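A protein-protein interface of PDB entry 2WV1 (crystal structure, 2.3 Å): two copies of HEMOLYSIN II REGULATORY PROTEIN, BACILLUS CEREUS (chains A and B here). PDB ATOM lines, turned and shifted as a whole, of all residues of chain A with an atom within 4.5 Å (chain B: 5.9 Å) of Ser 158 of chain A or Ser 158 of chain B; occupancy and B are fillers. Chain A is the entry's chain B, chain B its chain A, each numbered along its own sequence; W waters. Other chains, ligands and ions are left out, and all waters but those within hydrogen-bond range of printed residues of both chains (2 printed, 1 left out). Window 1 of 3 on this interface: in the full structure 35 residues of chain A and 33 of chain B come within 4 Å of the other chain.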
ATOM      1  N   TYR A 107      27.953  23.170  13.860  1.00  0.00           N
ATOM      2  CA  TYR A 107      28.131  22.246  12.775  1.00  0.00           C
ATOM      3  C   TYR A 107      28.260  23.036  11.490  1.00  0.00           C
ATOM      4  O   TYR A 107      28.912  22.574  10.561  1.00  0.00           O
ATOM      5  CB  TYR A 107      26.981  21.227  12.767  1.00  0.00           C
ATOM      6  CG  TYR A 107      27.199  19.950  11.982  1.00  0.00           C
ATOM      7  CD1 TYR A 107      27.439  18.741  12.626  1.00  0.00           C
ATOM      8  CD2 TYR A 107      27.108  19.944  10.600  1.00  0.00           C
ATOM      9  CE1 TYR A 107      27.614  17.573  11.905  1.00  0.00           C
ATOM     10  CE2 TYR A 107      27.279  18.789   9.878  1.00  0.00           C
ATOM     11  CZ  TYR A 107      27.529  17.616  10.525  1.00  0.00           C
ATOM     12  OH  TYR A 107      27.678  16.493   9.771  1.00  0.00           O
ATOM     13  N   HIS A 154      32.505   9.646  15.864  1.00  0.00           N
ATOM     14  CA  HIS A 154      32.003  10.361  14.721  1.00  0.00           C
ATOM     15  C   HIS A 154      30.491  10.247  14.595  1.00  0.00           C
ATOM     16  O   HIS A 154      29.810  11.267  14.516  1.00  0.00           O
ATOM     17  CB  HIS A 154      32.651   9.926  13.418  1.00  0.00           C
ATOM     18  CG  HIS A 154      32.014  10.565  12.229  1.00  0.00           C
ATOM     19  ND1 HIS A 154      31.060   9.929  11.462  1.00  0.00           N
ATOM     20  CD2 HIS A 154      32.139  11.816  11.720  1.00  0.00           C
ATOM     21  CE1 HIS A 154      30.648  10.750  10.512  1.00  0.00           C
ATOM     22  NE2 HIS A 154      31.286  11.900  10.646  1.00  0.00           N
ATOM     23  N   TRP A 155      29.956   9.026  14.560  1.00  0.00           N
ATOM     24  CA  TRP A 155      28.509   8.940  14.401  1.00  0.00           C
ATOM     25  C   TRP A 155      27.708   9.337  15.643  1.00  0.00           C
ATOM     26  O   TRP A 155      26.601   9.855  15.520  1.00  0.00           O
ATOM     27  CB  TRP A 155      28.025   7.634  13.754  1.00  0.00           C
ATOM     28  CG  TRP A 155      28.233   6.392  14.568  1.00  0.00           C
ATOM     29  CD1 TRP A 155      29.259   5.485  14.441  1.00  0.00           C
ATOM     30  CD2 TRP A 155      27.378   5.889  15.600  1.00  0.00           C
ATOM     31  NE1 TRP A 155      29.099   4.452  15.342  1.00  0.00           N
ATOM     32  CE2 TRP A 155      27.960   4.680  16.076  1.00  0.00           C
ATOM     33  CE3 TRP A 155      26.174   6.333  16.168  1.00  0.00           C
ATOM     34  CZ2 TRP A 155      27.379   3.912  17.097  1.00  0.00           C
ATOM     35  CZ3 TRP A 155      25.596   5.569  17.202  1.00  0.00           C
ATOM     36  CH2 TRP A 155      26.210   4.380  17.661  1.00  0.00           C
ATOM     37  N   ILE A 156      28.255   9.127  16.832  1.00  0.00           N
ATOM     38  CA  ILE A 156      27.563   9.569  18.044  1.00  0.00           C
ATOM     39  C   ILE A 156      27.522  11.100  18.139  1.00  0.00           C
ATOM     40  O   ILE A 156      26.488  11.664  18.469  1.00  0.00           O
ATOM     41  CB  ILE A 156      28.182   8.999  19.336  1.00  0.00           C
ATOM     42  CG1 ILE A 156      27.896   7.492  19.466  1.00  0.00           C
ATOM     43  CG2 ILE A 156      27.682   9.798  20.598  1.00  0.00           C
ATOM     44  CD1 ILE A 156      28.554   6.871  20.719  1.00  0.00           C
ATOM     45  N   THR A 157      28.637  11.781  17.880  1.00  0.00           N
ATOM     46  CA  THR A 157      28.594  13.233  17.938  1.00  0.00           C
ATOM     47  C   THR A 157      27.769  13.851  16.790  1.00  0.00           C
ATOM     48  O   THR A 157      27.180  14.930  16.964  1.00  0.00           O
ATOM     49  CB  THR A 157      29.987  13.840  18.009  1.00  0.00           C
ATOM     50  OG1 THR A 157      30.696  13.478  16.838  1.00  0.00           O
ATOM     51  CG2 THR A 157      30.749  13.313  19.227  1.00  0.00           C
ATOM     52  N   SER A 158      27.686  13.176  15.633  1.00  0.00           N
ATOM     53  CA  SER A 158      26.760  13.634  14.574  1.00  0.00           C
ATOM     54  C   SER A 158      25.324  13.648  15.063  1.00  0.00           C
ATOM     55  O   SER A 158      24.588  14.583  14.787  1.00  0.00           O
ATOM     56  CB  SER A 158      26.808  12.754  13.323  1.00  0.00           C
ATOM     57  OG  SER A 158      28.093  12.717  12.754  1.00  0.00           O
ATOM     58  N   ILE A 159      24.910  12.607  15.763  1.00  0.00           N
ATOM     59  CA  ILE A 159      23.560  12.570  16.319  1.00  0.00           C
ATOM     60  C   ILE A 159      23.369  13.671  17.366  1.00  0.00           C
ATOM     61  O   ILE A 159      22.357  14.365  17.349  1.00  0.00           O
ATOM     62  CB  ILE A 159      23.245  11.200  16.868  1.00  0.00           C
ATOM     63  CG1 ILE A 159      23.230  10.202  15.704  1.00  0.00           C
ATOM     64  CG2 ILE A 159      21.915  11.203  17.661  1.00  0.00           C
ATOM     65  CD1 ILE A 159      23.268   8.721  16.164  1.00  0.00           C
ATOM     66  N   VAL A 160      24.375  13.871  18.215  1.00  0.00           N
ATOM     67  CA  VAL A 160      24.299  14.864  19.279  1.00  0.00           C
ATOM     68  C   VAL A 160      24.240  16.290  18.737  1.00  0.00           C
ATOM     69  O   VAL A 160      23.355  17.076  19.113  1.00  0.00           O
ATOM     70  CB  VAL A 160      25.457  14.689  20.315  1.00  0.00           C
ATOM     71  CG1 VAL A 160      25.531  15.873  21.244  1.00  0.00           C
ATOM     72  CG2 VAL A 160      25.247  13.440  21.118  1.00  0.00           C
ATOM     73  N   LEU A 161      25.166  16.633  17.848  1.00  0.00           N
ATOM     74  CA  LEU A 161      25.203  17.992  17.276  1.00  0.00           C
ATOM     75  C   LEU A 161      24.240  18.221  16.112  1.00  0.00           C
ATOM     76  O   LEU A 161      23.838  19.359  15.877  1.00  0.00           O
ATOM     77  CB  LEU A 161      26.636  18.337  16.829  1.00  0.00           C
ATOM     78  CG  LEU A 161      27.651  18.242  17.952  1.00  0.00           C
ATOM     79  CD1 LEU A 161      29.055  18.369  17.400  1.00  0.00           C
ATOM     80  CD2 LEU A 161      27.335  19.345  18.972  1.00  0.00           C
ATOM     81  N   PHE A 162      23.890  17.154  15.385  1.00  0.00           N
ATOM     82  CA  PHE A 162      23.074  17.237  14.154  1.00  0.00           C
ATOM     83  C   PHE A 162      21.906  16.255  14.253  1.00  0.00           C
ATOM     84  O   PHE A 162      21.778  15.382  13.412  1.00  0.00           O
ATOM     85  CB  PHE A 162      23.948  16.866  12.937  1.00  0.00           C
ATOM     86  CG  PHE A 162      23.390  17.294  11.585  1.00  0.00           C
ATOM     87  CD1 PHE A 162      22.267  18.107  11.481  1.00  0.00           C
ATOM     88  CD2 PHE A 162      24.046  16.920  10.411  1.00  0.00           C
ATOM     89  CE1 PHE A 162      21.780  18.504  10.226  1.00  0.00           C
ATOM     90  CE2 PHE A 162      23.577  17.319   9.181  1.00  0.00           C
ATOM     91  CZ  PHE A 162      22.441  18.112   9.085  1.00  0.00           C
ATOM     92  N   PRO A 163      21.053  16.361  15.301  1.00  0.00           N
ATOM     93  CA  PRO A 163      19.965  15.357  15.420  1.00  0.00           C
ATOM     94  C   PRO A 163      19.008  15.374  14.219  1.00  0.00           C
ATOM     95  O   PRO A 163      18.396  14.357  13.903  1.00  0.00           O
ATOM     96  CB  PRO A 163      19.203  15.804  16.683  1.00  0.00           C
ATOM     97  CG  PRO A 163      19.563  17.331  16.825  1.00  0.00           C
ATOM     98  CD  PRO A 163      21.033  17.317  16.435  1.00  0.00           C
ATOM     99  N   PHE A 165      19.627  15.521  11.010  1.00  0.00           N
ATOM    100  CA  PHE A 165      20.092  14.643   9.953  1.00  0.00           C
ATOM    101  C   PHE A 165      19.598  13.250  10.242  1.00  0.00           C
ATOM    102  O   PHE A 165      19.103  12.563   9.341  1.00  0.00           O
ATOM    103  CB  PHE A 165      21.609  14.647   9.769  1.00  0.00           C
ATOM    104  CG  PHE A 165      22.040  13.992   8.486  1.00  0.00           C
ATOM    105  CD1 PHE A 165      21.628  14.512   7.255  1.00  0.00           C
ATOM    106  CD2 PHE A 165      22.801  12.822   8.501  1.00  0.00           C
ATOM    107  CE1 PHE A 165      21.998  13.896   6.052  1.00  0.00           C
ATOM    108  CE2 PHE A 165      23.177  12.192   7.305  1.00  0.00           C
ATOM    109  CZ  PHE A 165      22.785  12.730   6.079  1.00  0.00           C
ATOM    110  N   ILE B 153      23.099   3.626   6.948  1.00  0.00           N
ATOM    111  CA  ILE B 153      22.950   4.678   5.981  1.00  0.00           C
ATOM    112  C   ILE B 153      23.168   6.033   6.652  1.00  0.00           C
ATOM    113  O   ILE B 153      23.780   6.921   6.058  1.00  0.00           O
ATOM    114  CB  ILE B 153      21.596   4.564   5.270  1.00  0.00           C
ATOM    115  CG1 ILE B 153      21.681   3.403   4.277  1.00  0.00           C
ATOM    116  CG2 ILE B 153      21.202   5.883   4.564  1.00  0.00           C
ATOM    117  CD1 ILE B 153      20.367   3.091   3.587  1.00  0.00           C
ATOM    118  N   HIS B 154      22.705   6.179   7.897  1.00  0.00           N
ATOM    119  CA  HIS B 154      22.912   7.441   8.623  1.00  0.00           C
ATOM    120  C   HIS B 154      24.405   7.790   8.696  1.00  0.00           C
ATOM    121  O   HIS B 154      24.813   8.833   8.224  1.00  0.00           O
ATOM    122  CB  HIS B 154      22.311   7.432  10.025  1.00  0.00           C
ATOM    123  CG  HIS B 154      22.774   8.584  10.855  1.00  0.00           C
ATOM    124  ND1 HIS B 154      23.877   8.506  11.679  1.00  0.00           N
ATOM    125  CD2 HIS B 154      22.348   9.871  10.911  1.00  0.00           C
ATOM    126  CE1 HIS B 154      24.079   9.683  12.247  1.00  0.00           C
ATOM    127  NE2 HIS B 154      23.187  10.537  11.773  1.00  0.00           N
ATOM    128  N   TRP B 155      25.229   6.905   9.244  1.00  0.00           N
ATOM    129  CA  TRP B 155      26.642   7.275   9.403  1.00  0.00           C
ATOM    130  C   TRP B 155      27.417   7.374   8.065  1.00  0.00           C
ATOM    131  O   TRP B 155      28.272   8.246   7.907  1.00  0.00           O
ATOM    132  CB  TRP B 155      27.350   6.436  10.491  1.00  0.00           C
ATOM    133  CG  TRP B 155      27.579   4.974  10.190  1.00  0.00           C
ATOM    134  CD1 TRP B 155      26.849   3.923  10.657  1.00  0.00           C
ATOM    135  CD2 TRP B 155      28.650   4.404   9.416  1.00  0.00           C
ATOM    136  NE1 TRP B 155      27.380   2.733  10.211  1.00  0.00           N
ATOM    137  CE2 TRP B 155      28.478   2.997   9.437  1.00  0.00           C
ATOM    138  CE3 TRP B 155      29.730   4.948   8.694  1.00  0.00           C
ATOM    139  CZ2 TRP B 155      29.348   2.109   8.750  1.00  0.00           C
ATOM    140  CZ3 TRP B 155      30.604   4.070   8.014  1.00  0.00           C
ATOM    141  CH2 TRP B 155      30.405   2.665   8.047  1.00  0.00           C
ATOM    142  N   ILE B 156      27.096   6.520   7.093  1.00  0.00           N
ATOM    143  CA  ILE B 156      27.758   6.608   5.769  1.00  0.00           C
ATOM    144  C   ILE B 156      27.413   7.916   5.063  1.00  0.00           C
ATOM    145  O   ILE B 156      28.308   8.636   4.626  1.00  0.00           O
ATOM    146  CB  ILE B 156      27.391   5.417   4.829  1.00  0.00           C
ATOM    147  CG1 ILE B 156      27.901   4.079   5.375  1.00  0.00           C
ATOM    148  CG2 ILE B 156      27.882   5.660   3.421  1.00  0.00           C
ATOM    149  CD1 ILE B 156      27.394   2.879   4.504  1.00  0.00           C
ATOM    150  N   THR B 157      26.120   8.222   4.945  1.00  0.00           N
ATOM    151  CA  THR B 157      25.717   9.452   4.264  1.00  0.00           C
ATOM    152  C   THR B 157      26.195  10.669   5.033  1.00  0.00           C
ATOM    153  O   THR B 157      26.340  11.742   4.467  1.00  0.00           O
ATOM    154  CB  THR B 157      24.197   9.539   4.031  1.00  0.00           C
ATOM    155  OG1 THR B 157      23.521   9.389   5.287  1.00  0.00           O
ATOM    156  CG2 THR B 157      23.751   8.448   3.077  1.00  0.00           C
ATOM    157  N   SER B 158      26.460  10.499   6.323  1.00  0.00           N
ATOM    158  CA  SER B 158      26.998  11.595   7.105  1.00  0.00           C
ATOM    159  C   SER B 158      28.402  11.951   6.625  1.00  0.00           C
ATOM    160  O   SER B 158      28.708  13.129   6.452  1.00  0.00           O
ATOM    161  CB  SER B 158      27.004  11.282   8.598  1.00  0.00           C
ATOM    162  OG  SER B 158      27.316  12.466   9.300  1.00  0.00           O
ATOM    163  N   ILE B 159      29.237  10.933   6.392  1.00  0.00           N
ATOM    164  CA  ILE B 159      30.615  11.117   5.910  1.00  0.00           C
ATOM    165  C   ILE B 159      30.601  11.696   4.511  1.00  0.00           C
ATOM    166  O   ILE B 159      31.354  12.596   4.209  1.00  0.00           O
ATOM    167  CB  ILE B 159      31.367   9.784   5.863  1.00  0.00           C
ATOM    168  CG1 ILE B 159      31.629   9.291   7.294  1.00  0.00           C
ATOM    169  CG2 ILE B 159      32.681   9.900   5.018  1.00  0.00           C
ATOM    170  CD1 ILE B 159      32.002   7.824   7.402  1.00  0.00           C
ATOM    171  N   VAL B 160      29.702  11.180   3.681  1.00  0.00           N
ATOM    172  CA  VAL B 160      29.563  11.576   2.294  1.00  0.00           C
ATOM    173  C   VAL B 160      29.094  13.020   2.098  1.00  0.00           C
ATOM    174  O   VAL B 160      29.689  13.771   1.308  1.00  0.00           O
ATOM    175  CB  VAL B 160      28.603  10.583   1.542  1.00  0.00           C
ATOM    176  CG1 VAL B 160      28.088  11.173   0.268  1.00  0.00           C
ATOM    177  CG2 VAL B 160      29.316   9.262   1.258  1.00  0.00           C
ATOM    178  N   LEU B 161      28.008  13.402   2.770  1.00  0.00           N
ATOM    179  CA  LEU B 161      27.490  14.750   2.593  1.00  0.00           C
ATOM    180  C   LEU B 161      28.224  15.783   3.413  1.00  0.00           C
ATOM    181  O   LEU B 161      28.139  16.955   3.123  1.00  0.00           O
ATOM    182  CB  LEU B 161      26.021  14.810   2.970  1.00  0.00           C
ATOM    183  CG  LEU B 161      25.064  14.090   2.048  1.00  0.00           C
ATOM    184  CD1 LEU B 161      23.659  14.254   2.616  1.00  0.00           C
ATOM    185  CD2 LEU B 161      25.188  14.657   0.622  1.00  0.00           C
ATOM    186  N   PHE B 162      28.899  15.343   4.464  1.00  0.00           N
ATOM    187  CA  PHE B 162      29.533  16.250   5.414  1.00  0.00           C
ATOM    188  C   PHE B 162      30.946  15.769   5.734  1.00  0.00           C
ATOM    189  O   PHE B 162      31.318  15.590   6.910  1.00  0.00           O
ATOM    190  CB  PHE B 162      28.667  16.391   6.678  1.00  0.00           C
ATOM    191  CG  PHE B 162      27.241  16.763   6.387  1.00  0.00           C
ATOM    192  CD1 PHE B 162      26.929  18.024   5.900  1.00  0.00           C
ATOM    193  CD2 PHE B 162      26.215  15.855   6.583  1.00  0.00           C
ATOM    194  CE1 PHE B 162      25.619  18.383   5.614  1.00  0.00           C
ATOM    195  CE2 PHE B 162      24.887  16.204   6.304  1.00  0.00           C
ATOM    196  CZ  PHE B 162      24.596  17.462   5.820  1.00  0.00           C
ATOM    197  N   PRO B 163      31.771  15.577   4.676  1.00  0.00           N
ATOM    198  CA  PRO B 163      33.154  15.124   4.888  1.00  0.00           C
ATOM    199  C   PRO B 163      33.902  15.992   5.869  1.00  0.00           C
ATOM    200  O   PRO B 163      34.798  15.516   6.502  1.00  0.00           O
ATOM    201  CB  PRO B 163      33.816  15.283   3.496  1.00  0.00           C
ATOM    202  CG  PRO B 163      32.972  16.378   2.818  1.00  0.00           C
ATOM    203  CD  PRO B 163      31.563  16.050   3.290  1.00  0.00           C
ATOM    204  N   PHE B 165      33.073  17.329   8.770  1.00  0.00           N
ATOM    205  CA  PHE B 165      32.856  16.945  10.165  1.00  0.00           C
ATOM    206  C   PHE B 165      33.654  15.699  10.456  1.00  0.00           C
ATOM    207  O   PHE B 165      34.226  15.564  11.523  1.00  0.00           O
ATOM    208  CB  PHE B 165      31.376  16.674  10.457  1.00  0.00           C
ATOM    209  CG  PHE B 165      31.073  16.434  11.909  1.00  0.00           C
ATOM    210  CD1 PHE B 165      31.170  17.468  12.841  1.00  0.00           C
ATOM    211  CD2 PHE B 165      30.692  15.173  12.348  1.00  0.00           C
ATOM    212  CE1 PHE B 165      30.885  17.248  14.180  1.00  0.00           C
ATOM    213  CE2 PHE B 165      30.398  14.949  13.682  1.00  0.00           C
ATOM    214  CZ  PHE B 165      30.499  15.986  14.602  1.00  0.00           C
HETATM  215  O   HOH W   1      23.196  13.129  12.512  1.00  0.00           O
HETATM  216  O   HOH W   2      30.025  13.596   8.791  1.00  0.00           O
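The backbone carbonyl oxygen (O) of Ile 153 of chain B sits at hydrogen-bond distance from the side-chain hydroxyl (OG1) of Thr 157 of chain B, 2.6 Å away. OG1 of Thr 157 of chain B lies within hydrogen-bond range of O of His 154 of chain B, 3.3 Å away. The backbone carbonyl oxygen of His 154 of chain A sits at hydrogen-bond distance from the side-chain hydroxyl of Thr 157 of chain A (3.3 Å). OG of Ser 158 of chain A lies within hydrogen-bond range of O of His 154 of chain A (2.9 Å).
His 154 of chain A touches Ser 158 of chain B, but with the chains exchanged Ser 158 of chain A does not touch His 154 of chain B (4.2 Å). His 154 of chain A touches Ile 159 of chain B, and with the chains exchanged Ile 159 of chain A touches His 154 of chain B. Ser 158 of chain A touches Phe 165 of chain B, and with the chains exchanged Phe 165 of chain A touches Ser 158 of chain B. Leu 161 of chain A touches Phe 165 of chain B, and with the chains exchanged Phe 165 of chain A touches Leu 161 of chain B. 11 positions are printed for both chains.
Among the printed residues, merely in contact across the chains: Tyr 107 of chain A with Phe 162 of chain B (3.2 Å), Ser 158 of chain A with Phe 165 of chain B (3.3 Å), Phe 162 of chain A with Phe 162 of chain B (3.4 Å), Thr 157 of chain A with Phe 165 of chain B (3.4 Å), Phe 165 of chain A with Thr 157 of chain B (3.5 Å), Trp 155 of chain A with Trp 155 of chain B (3.5 Å), Ser 158 of chain A with Ser 158 of chain B (3.5 Å), Ile 159 of chain A with His 154 of chain B (3.6 Å), Tyr 107 of chain A with Phe 165 of chain B (3.6 Å), His 154 of chain A with Ile 159 of chain B (3.7 Å), Phe 165 of chain A with Phe 162 of chain B (3.7 Å), His 154 of chain A with Phe 165 of chain B (3.7 Å), Phe 165 of chain A with Ser 158 of chain B (3.8 Å), Phe 165 of chain A with Leu 161 of chain B (3.8 Å), Phe 165 of chain A with His 154 of chain B (3.8 Å), Leu 161 of chain A with Phe 165 of chain B (3.9 Å) and His 154 of chain A with Ser 158 of chain B (3.9 Å).
Of the 12 printed residues of chain A, 9 touch a printed residue of chain B. Printed residues of chain A that touch a printed residue of chain B: Tyr 107, His 154, Trp 155, Thr 157, Ser 158, Ile 159, Leu 161, Phe 162 and Phe 165. Printed residues of chain B that touch a printed residue of chain A: His 154, Trp 155, Thr 157, Ser 158, Ile 159, Leu 161, Phe 162 and Phe 165. Hydrophobic or aromatic side chains of chain B that line the printed part of chain A: His 154, Trp 155, Ile 159, Leu 161, Phe 162 and Phe 165. Among the printed residues, no Asp or Glu carboxylate lies within 4 Å of a Lys or Arg side-chain nitrogen of the other chain.
Printed residues of chain B within 4 Å of Trp 155 of chain A: Trp 155. Printed residues of chain B within 4 Å of Ser 158 of chain A: Ser 158 (3.5 Å) and Phe 165 (3.3 Å). Printed residues of chain B within 4 Å of Ile 159 of chain A: His 154. Pro 163 of chain A touches none of the printed residues of chain B. Printed residues of chain B within 4 Å of Phe 165 of chain A: His 154 (3.8 Å), Thr 157 (3.5 Å), Ser 158 (3.8 Å), Leu 161 (3.8 Å) and Phe 162 (3.7 Å). Of the printed residues of chain A, Trp 155 of chain B touches Trp 155 (3.5 Å).
Water W1 lies within hydrogen-bond range of NE2 of His 154 of chain B (2.7 Å), O of Phe 162 of chain A (2.8 Å) and O of Ser 158 of chain A (3.0 Å). Water W2 lies within hydrogen-bond range of O of Ser 158 of chain B, NE2 of His 154 of chain A and O of Phe 162 of chain B.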
